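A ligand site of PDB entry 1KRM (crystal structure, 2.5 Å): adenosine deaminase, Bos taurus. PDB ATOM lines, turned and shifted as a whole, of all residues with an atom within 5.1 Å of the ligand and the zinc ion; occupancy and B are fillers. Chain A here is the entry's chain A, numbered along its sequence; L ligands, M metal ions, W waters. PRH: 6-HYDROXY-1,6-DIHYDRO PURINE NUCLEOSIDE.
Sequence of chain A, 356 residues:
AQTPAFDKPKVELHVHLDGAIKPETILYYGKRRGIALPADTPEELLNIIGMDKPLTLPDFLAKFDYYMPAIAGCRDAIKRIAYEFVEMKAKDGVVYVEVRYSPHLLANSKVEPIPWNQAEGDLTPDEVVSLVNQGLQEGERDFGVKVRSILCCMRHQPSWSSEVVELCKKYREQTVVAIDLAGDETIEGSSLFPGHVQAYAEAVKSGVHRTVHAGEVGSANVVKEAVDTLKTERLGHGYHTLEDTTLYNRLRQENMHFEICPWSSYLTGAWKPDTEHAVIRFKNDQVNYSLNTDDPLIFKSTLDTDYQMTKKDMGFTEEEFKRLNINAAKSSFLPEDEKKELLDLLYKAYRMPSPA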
ATOM      1  N   HIS A  14      -4.566   6.646 -18.782  1.00  0.00           N
ATOM      2  CA  HIS A  14      -4.599   8.113 -18.580  1.00  0.00           C
ATOM      3  C   HIS A  14      -5.379   8.901 -19.618  1.00  0.00           C
ATOM      4  O   HIS A  14      -4.833   9.297 -20.647  1.00  0.00           O
ATOM      5  CB  HIS A  14      -3.173   8.750 -18.444  1.00  0.00           C
ATOM      6  CG  HIS A  14      -3.050  10.157 -17.824  1.00  0.00           C
ATOM      7  ND1 HIS A  14      -2.482  10.379 -16.636  1.00  0.00           N
ATOM      8  CD2 HIS A  14      -3.338  11.434 -18.368  1.00  0.00           C
ATOM      9  CE1 HIS A  14      -2.388  11.732 -16.458  1.00  0.00           C
ATOM     10  NE2 HIS A  14      -2.934  12.416 -17.519  1.00  0.00           N
ATOM     11  N   HIS A  16      -8.484  12.260 -20.066  1.00  0.00           N
ATOM     12  CA  HIS A  16      -9.451  13.045 -19.341  1.00  0.00           C
ATOM     13  C   HIS A  16     -10.764  13.290 -20.105  1.00  0.00           C
ATOM     14  O   HIS A  16     -10.785  13.990 -21.122  1.00  0.00           O
ATOM     15  CB  HIS A  16      -8.785  14.369 -18.887  1.00  0.00           C
ATOM     16  CG  HIS A  16      -7.505  14.227 -18.025  1.00  0.00           C
ATOM     17  ND1 HIS A  16      -7.317  14.892 -16.882  1.00  0.00           N
ATOM     18  CD2 HIS A  16      -6.292  13.580 -18.288  1.00  0.00           C
ATOM     19  CE1 HIS A  16      -6.061  14.695 -16.439  1.00  0.00           C
ATOM     20  NE2 HIS A  16      -5.394  13.898 -17.315  1.00  0.00           N
ATOM     21  N   ASP A  18     -13.179  15.638 -19.642  1.00  0.00           N
ATOM     22  CA  ASP A  18     -12.756  17.024 -19.886  1.00  0.00           C
ATOM     23  C   ASP A  18     -12.307  17.401 -21.272  1.00  0.00           C
ATOM     24  O   ASP A  18     -12.895  18.267 -21.850  1.00  0.00           O
ATOM     25  CB  ASP A  18     -11.568  17.206 -18.968  1.00  0.00           C
ATOM     26  CG  ASP A  18     -11.963  17.972 -17.728  1.00  0.00           C
ATOM     27  OD1 ASP A  18     -12.905  17.600 -17.013  1.00  0.00           O
ATOM     28  OD2 ASP A  18     -11.300  18.975 -17.493  1.00  0.00           O
ATOM     29  N   LEU A  57       2.774  23.936 -19.988  1.00  0.00           N
ATOM     30  CA  LEU A  57       1.675  23.404 -19.179  1.00  0.00           C
ATOM     31  C   LEU A  57       0.650  24.405 -18.673  1.00  0.00           C
ATOM     32  O   LEU A  57      -0.561  24.187 -18.829  1.00  0.00           O
ATOM     33  CB  LEU A  57       2.208  22.619 -17.978  1.00  0.00           C
ATOM     34  CG  LEU A  57       1.076  21.965 -17.178  1.00  0.00           C
ATOM     35  CD1 LEU A  57       0.724  20.657 -17.859  1.00  0.00           C
ATOM     36  CD2 LEU A  57       1.328  21.830 -15.666  1.00  0.00           C
ATOM     37  N   PHE A  60      -1.541  25.202 -21.794  1.00  0.00           N
ATOM     38  CA  PHE A  60      -2.433  24.013 -21.987  1.00  0.00           C
ATOM     39  C   PHE A  60      -3.776  24.124 -21.260  1.00  0.00           C
ATOM     40  O   PHE A  60      -4.857  24.082 -21.844  1.00  0.00           O
ATOM     41  CB  PHE A  60      -1.714  22.673 -21.617  1.00  0.00           C
ATOM     42  CG  PHE A  60      -2.622  21.449 -21.622  1.00  0.00           C
ATOM     43  CD1 PHE A  60      -3.020  20.845 -22.829  1.00  0.00           C
ATOM     44  CD2 PHE A  60      -3.095  20.945 -20.400  1.00  0.00           C
ATOM     45  CE1 PHE A  60      -3.972  19.814 -22.813  1.00  0.00           C
ATOM     46  CE2 PHE A  60      -4.028  19.892 -20.378  1.00  0.00           C
ATOM     47  CZ  PHE A  60      -4.479  19.357 -21.592  1.00  0.00           C
ATOM     48  N   LEU A  61      -3.584  24.371 -19.943  1.00  0.00           N
ATOM     49  CA  LEU A  61      -4.610  24.349 -18.893  1.00  0.00           C
ATOM     50  C   LEU A  61      -5.703  25.391 -18.871  1.00  0.00           C
ATOM     51  O   LEU A  61      -6.686  25.293 -18.125  1.00  0.00           O
ATOM     52  CB  LEU A  61      -3.887  24.276 -17.537  1.00  0.00           C
ATOM     53  CG  LEU A  61      -3.646  22.814 -17.361  1.00  0.00           C
ATOM     54  CD1 LEU A  61      -2.268  22.469 -16.872  1.00  0.00           C
ATOM     55  CD2 LEU A  61      -4.771  22.239 -16.582  1.00  0.00           C
ATOM     56  N   PHE A  64      -8.721  24.975 -22.149  1.00  0.00           N
ATOM     57  CA  PHE A  64      -9.931  24.639 -21.399  1.00  0.00           C
ATOM     58  C   PHE A  64     -10.936  25.698 -21.052  1.00  0.00           C
ATOM     59  O   PHE A  64     -12.104  25.420 -20.843  1.00  0.00           O
ATOM     60  CB  PHE A  64      -9.573  24.006 -20.079  1.00  0.00           C
ATOM     61  CG  PHE A  64      -9.108  22.604 -20.272  1.00  0.00           C
ATOM     62  CD1 PHE A  64      -7.839  22.356 -20.834  1.00  0.00           C
ATOM     63  CD2 PHE A  64      -9.954  21.570 -19.871  1.00  0.00           C
ATOM     64  CE1 PHE A  64      -7.381  21.045 -20.999  1.00  0.00           C
ATOM     65  CE2 PHE A  64      -9.486  20.270 -20.009  1.00  0.00           C
ATOM     66  CZ  PHE A  64      -8.223  20.020 -20.578  1.00  0.00           C
ATOM     67  N   ARG A 100     -10.412   9.606 -16.319  1.00  0.00           N
ATOM     68  CA  ARG A 100     -10.540  10.563 -15.220  1.00  0.00           C
ATOM     69  C   ARG A 100     -11.279  11.822 -15.531  1.00  0.00           C
ATOM     70  O   ARG A 100     -11.346  12.280 -16.652  1.00  0.00           O
ATOM     71  CB  ARG A 100      -9.197  10.928 -14.565  1.00  0.00           C
ATOM     72  CG  ARG A 100      -8.201  11.754 -15.408  1.00  0.00           C
ATOM     73  CD  ARG A 100      -6.750  11.572 -14.931  1.00  0.00           C
ATOM     74  NE  ARG A 100      -6.441  10.146 -14.904  1.00  0.00           N
ATOM     75  CZ  ARG A 100      -5.202   9.665 -14.723  1.00  0.00           C
ATOM     76  NH1 ARG A 100      -5.057   8.362 -14.901  1.00  0.00           N
ATOM     77  NH2 ARG A 100      -4.172  10.391 -14.396  1.00  0.00           N
ATOM     78  N   TYR A 101     -11.803  12.388 -14.448  1.00  0.00           N
ATOM     79  CA  TYR A 101     -12.428  13.721 -14.542  1.00  0.00           C
ATOM     80  C   TYR A 101     -12.558  14.513 -13.248  1.00  0.00           C
ATOM     81  O   TYR A 101     -12.205  14.085 -12.159  1.00  0.00           O
ATOM     82  CB  TYR A 101     -13.761  13.762 -15.324  1.00  0.00           C
ATOM     83  CG  TYR A 101     -14.914  13.058 -14.638  1.00  0.00           C
ATOM     84  CD1 TYR A 101     -15.860  13.788 -13.884  1.00  0.00           C
ATOM     85  CD2 TYR A 101     -15.021  11.664 -14.790  1.00  0.00           C
ATOM     86  CE1 TYR A 101     -16.842  13.089 -13.193  1.00  0.00           C
ATOM     87  CE2 TYR A 101     -16.022  10.972 -14.113  1.00  0.00           C
ATOM     88  CZ  TYR A 101     -16.839  11.698 -13.262  1.00  0.00           C
ATOM     89  OH  TYR A 101     -17.616  10.967 -12.420  1.00  0.00           O
ATOM     90  N   SER A 102     -13.074  15.724 -13.390  1.00  0.00           N
ATOM     91  CA  SER A 102     -13.158  16.567 -12.192  1.00  0.00           C
ATOM     92  C   SER A 102     -14.527  17.127 -11.821  1.00  0.00           C
ATOM     93  O   SER A 102     -14.842  18.223 -12.237  1.00  0.00           O
ATOM     94  CB  SER A 102     -12.238  17.762 -12.321  1.00  0.00           C
ATOM     95  OG  SER A 102     -12.299  18.543 -11.107  1.00  0.00           O
ATOM     96  N   LEU A 105     -14.936  20.815 -11.809  1.00  0.00           N
ATOM     97  CA  LEU A 105     -15.223  21.607 -13.029  1.00  0.00           C
ATOM     98  C   LEU A 105     -16.666  21.591 -13.672  1.00  0.00           C
ATOM     99  O   LEU A 105     -17.118  22.428 -14.447  1.00  0.00           O
ATOM    100  CB  LEU A 105     -14.152  21.224 -13.986  1.00  0.00           C
ATOM    101  CG  LEU A 105     -12.744  21.321 -13.464  1.00  0.00           C
ATOM    102  CD1 LEU A 105     -11.827  21.250 -14.674  1.00  0.00           C
ATOM    103  CD2 LEU A 105     -12.466  22.660 -12.760  1.00  0.00           C
ATOM    104  N   CYS A 152     -10.954  13.224  -9.854  1.00  0.00           N
ATOM    105  CA  CYS A 152      -9.695  13.932  -9.726  1.00  0.00           C
ATOM    106  C   CYS A 152      -9.746  15.042  -8.760  1.00  0.00           C
ATOM    107  O   CYS A 152     -10.318  16.076  -9.061  1.00  0.00           O
ATOM    108  CB  CYS A 152      -9.366  14.730 -10.948  1.00  0.00           C
ATOM    109  SG  CYS A 152      -8.182  13.889 -11.886  1.00  0.00           S
ATOM    110  N   MET A 154      -7.951  18.331  -7.441  1.00  0.00           N
ATOM    111  CA  MET A 154      -7.457  19.254  -8.441  1.00  0.00           C
ATOM    112  C   MET A 154      -6.489  20.249  -7.809  1.00  0.00           C
ATOM    113  O   MET A 154      -6.935  20.978  -6.904  1.00  0.00           O
ATOM    114  CB  MET A 154      -8.731  19.899  -8.854  1.00  0.00           C
ATOM    115  CG  MET A 154      -8.605  20.783 -10.033  1.00  0.00           C
ATOM    116  SD  MET A 154      -8.800  19.786 -11.470  1.00  0.00           S
ATOM    117  CE  MET A 154      -8.814  21.284 -12.429  1.00  0.00           C
ATOM    118  N   ALA A 182      -4.742  16.604 -10.125  1.00  0.00           N
ATOM    119  CA  ALA A 182      -4.461  17.106 -11.497  1.00  0.00           C
ATOM    120  C   ALA A 182      -4.466  18.612 -11.711  1.00  0.00           C
ATOM    121  O   ALA A 182      -4.959  19.286 -10.841  1.00  0.00           O
ATOM    122  CB  ALA A 182      -5.465  16.536 -12.468  1.00  0.00           C
ATOM    123  N   GLY A 183      -3.931  19.154 -12.810  1.00  0.00           N
ATOM    124  CA  GLY A 183      -3.811  20.627 -12.820  1.00  0.00           C
ATOM    125  C   GLY A 183      -2.347  21.066 -12.845  1.00  0.00           C
ATOM    126  O   GLY A 183      -1.532  20.173 -12.973  1.00  0.00           O
ATOM    127  N   HIS A 213      -0.691  12.997 -10.902  1.00  0.00           N
ATOM    128  CA  HIS A 213       0.175  13.461 -11.992  1.00  0.00           C
ATOM    129  C   HIS A 213       1.462  14.128 -11.534  1.00  0.00           C
ATOM    130  O   HIS A 213       1.527  15.328 -11.359  1.00  0.00           O
ATOM    131  CB  HIS A 213      -0.407  14.567 -12.863  1.00  0.00           C
ATOM    132  CG  HIS A 213      -1.588  14.258 -13.767  1.00  0.00           C
ATOM    133  ND1 HIS A 213      -2.769  13.776 -13.354  1.00  0.00           N
ATOM    134  CD2 HIS A 213      -1.719  14.622 -15.112  1.00  0.00           C
ATOM    135  CE1 HIS A 213      -3.620  13.850 -14.427  1.00  0.00           C
ATOM    136  NE2 HIS A 213      -2.998  14.376 -15.539  1.00  0.00           N
ATOM    137  N   GLU A 216       5.855  14.968 -15.196  1.00  0.00           N
ATOM    138  CA  GLU A 216       5.466  15.947 -16.250  1.00  0.00           C
ATOM    139  C   GLU A 216       6.268  17.258 -16.323  1.00  0.00           C
ATOM    140  O   GLU A 216       7.435  17.209 -16.668  1.00  0.00           O
ATOM    141  CB  GLU A 216       3.929  16.131 -16.212  1.00  0.00           C
ATOM    142  CG  GLU A 216       3.156  16.781 -17.381  1.00  0.00           C
ATOM    143  CD  GLU A 216       1.723  17.102 -16.993  1.00  0.00           C
ATOM    144  OE1 GLU A 216       1.391  16.987 -15.825  1.00  0.00           O
ATOM    145  OE2 GLU A 216       0.963  17.489 -17.863  1.00  0.00           O
ATOM    146  N   HIS A 237       2.475  10.118 -14.984  1.00  0.00           N
ATOM    147  CA  HIS A 237       3.480  10.682 -15.915  1.00  0.00           C
ATOM    148  C   HIS A 237       4.957  10.458 -15.524  1.00  0.00           C
ATOM    149  O   HIS A 237       5.756   9.837 -16.223  1.00  0.00           O
ATOM    150  CB  HIS A 237       3.383  12.172 -16.236  1.00  0.00           C
ATOM    151  CG  HIS A 237       2.422  12.709 -17.289  1.00  0.00           C
ATOM    152  ND1 HIS A 237       2.703  12.833 -18.594  1.00  0.00           N
ATOM    153  CD2 HIS A 237       1.215  13.361 -17.060  1.00  0.00           C
ATOM    154  CE1 HIS A 237       1.736  13.555 -19.169  1.00  0.00           C
ATOM    155  NE2 HIS A 237       0.805  13.878 -18.213  1.00  0.00           N
ATOM    156  N   ASP A 294      -4.293  11.096 -22.770  1.00  0.00           N
ATOM    157  CA  ASP A 294      -4.377  12.317 -21.979  1.00  0.00           C
ATOM    158  C   ASP A 294      -5.430  13.320 -22.422  1.00  0.00           C
ATOM    159  O   ASP A 294      -6.461  13.466 -21.805  1.00  0.00           O
ATOM    160  CB  ASP A 294      -2.967  12.877 -21.896  1.00  0.00           C
ATOM    161  CG  ASP A 294      -2.662  13.879 -20.809  1.00  0.00           C
ATOM    162  OD1 ASP A 294      -3.436  13.950 -19.880  1.00  0.00           O
ATOM    163  OD2 ASP A 294      -1.629  14.558 -20.901  1.00  0.00           O
ATOM    164  N   ASP A 295      -5.166  13.974 -23.538  1.00  0.00           N
ATOM    165  CA  ASP A 295      -6.261  14.798 -24.043  1.00  0.00           C
ATOM    166  C   ASP A 295      -6.492  14.839 -25.540  1.00  0.00           C
ATOM    167  O   ASP A 295      -6.196  15.831 -26.197  1.00  0.00           O
ATOM    168  CB  ASP A 295      -6.104  16.270 -23.732  1.00  0.00           C
ATOM    169  CG  ASP A 295      -6.040  16.597 -22.296  1.00  0.00           C
ATOM    170  OD1 ASP A 295      -6.955  17.264 -21.816  1.00  0.00           O
ATOM    171  OD2 ASP A 295      -5.062  16.220 -21.639  1.00  0.00           O
HETATM  172  N1  PRH L   1      -1.372  16.999 -16.863  1.00  0.00           N
HETATM  173  C2  PRH L   1      -1.782  18.203 -16.240  1.00  0.00           C
HETATM  174  N3  PRH L   1      -3.060  18.596 -16.236  1.00  0.00           N
HETATM  175  C4  PRH L   1      -3.867  17.817 -17.106  1.00  0.00           C
HETATM  176  C5  PRH L   1      -3.329  16.884 -17.974  1.00  0.00           C
HETATM  177  C6  PRH L   1      -1.906  16.649 -18.129  1.00  0.00           C
HETATM  178  O6  PRH L   1      -1.730  15.202 -18.133  1.00  0.00           O
HETATM  179  N7  PRH L   1      -4.279  16.291 -18.644  1.00  0.00           N
HETATM  180  C8  PRH L   1      -5.403  16.929 -18.208  1.00  0.00           C
HETATM  181  N9  PRH L   1      -5.180  17.824 -17.231  1.00  0.00           N
HETATM  182  C1' PRH L   1      -6.151  18.450 -16.298  1.00  0.00           C
HETATM  183  C2' PRH L   1      -7.159  19.528 -16.684  1.00  0.00           C
HETATM  184  O2' PRH L   1      -7.081  20.632 -15.675  1.00  0.00           O
HETATM  185  C3' PRH L   1      -8.508  18.906 -16.282  1.00  0.00           C
HETATM  186  O3' PRH L   1      -9.491  19.735 -15.587  1.00  0.00           O
HETATM  187  C4' PRH L   1      -8.056  17.976 -15.203  1.00  0.00           C
HETATM  188  O4' PRH L   1      -6.987  17.403 -15.873  1.00  0.00           O
HETATM  189  C5' PRH L   1      -9.054  16.942 -14.743  1.00  0.00           C
HETATM  190  O5' PRH L   1      -9.544  16.285 -16.015  1.00  0.00           O
HETATM  191 ZN    ZN M   1      -3.357  14.402 -17.706  1.00  0.00          ZN
HETATM  192  O   HOH W   1       0.236  18.030 -13.443  1.00  0.00           O
HETATM  193  O   HOH W   2      -8.974  22.532 -15.161  1.00  0.00           O
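N1 of the ligand sits at hydrogen-bond distance from OE2 of Glu 216, 2.6 Å away.
The side-chain carboxylate (OD2) of Asp 18 lies within hydrogen-bond range of an oxygen (O3') of the ligand, 2.7 Å away.
An oxygen (O6) of the ligand lies close to a ring nitrogen (NE2) of His 237 (2.9 Å).
OD2 of Asp 295 sits close to N7 of the ligand (3.1 Å).
Merely in contact with the ligand: Leu 57 (3.9 Å), Phe 60 (3.9 Å), Leu 61 (3.0 Å), Leu 105 (2.9 Å), Met 154 (3.6 Å), Ala 182 (3.8 Å) and Gly 183 (3.6 Å).
Hydrophobic or aromatic side chains that line the ligand: His 14, His 16, Leu 57, Phe 60, Leu 61, Leu 105, Met 154, Ala 182, His 213 and His 237.
Within 4 Å of the ligand: His 14, His 16, Asp 18, Leu 57, Phe 60, Leu 61, Leu 105, Met 154, Ala 182, Gly 183, His 213, Glu 216, His 237, Asp 294 and Asp 295.
Four residues have an atom within 4 Å of the zinc ion: His 14, His 16, His 213 and Asp 294.
Along chain A the residues within 4 Å of the zinc ion span positions 14 to 294.
The nearest printed residue that does not touch the zinc ion is His 237 (4.2 Å).
Water W1 bridges O of Gly 183 (2.8 Å) and OE1 of Glu 216 (2.8 Å).
The zinc ion is bound by O6 of the ligand (1.9 Å), NE2 of His 14 (2.0 Å), NE2 of His 16 (2.1 Å), NE2 of His 213 (2.2 Å), OD1 of Asp 294 (2.2 Å) and N7 of the ligand (2.3 Å).
The guanidinium group (NH2) of Arg 100 is in hydrogen-bond range of a ring nitrogen (ND1) of His 14 (2.8 Å).
The side-chain sulfur (SD) of Met 154 is in hydrogen-bond range of the side-chain hydroxyl (OG) of Ser 102 (3.7 Å).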
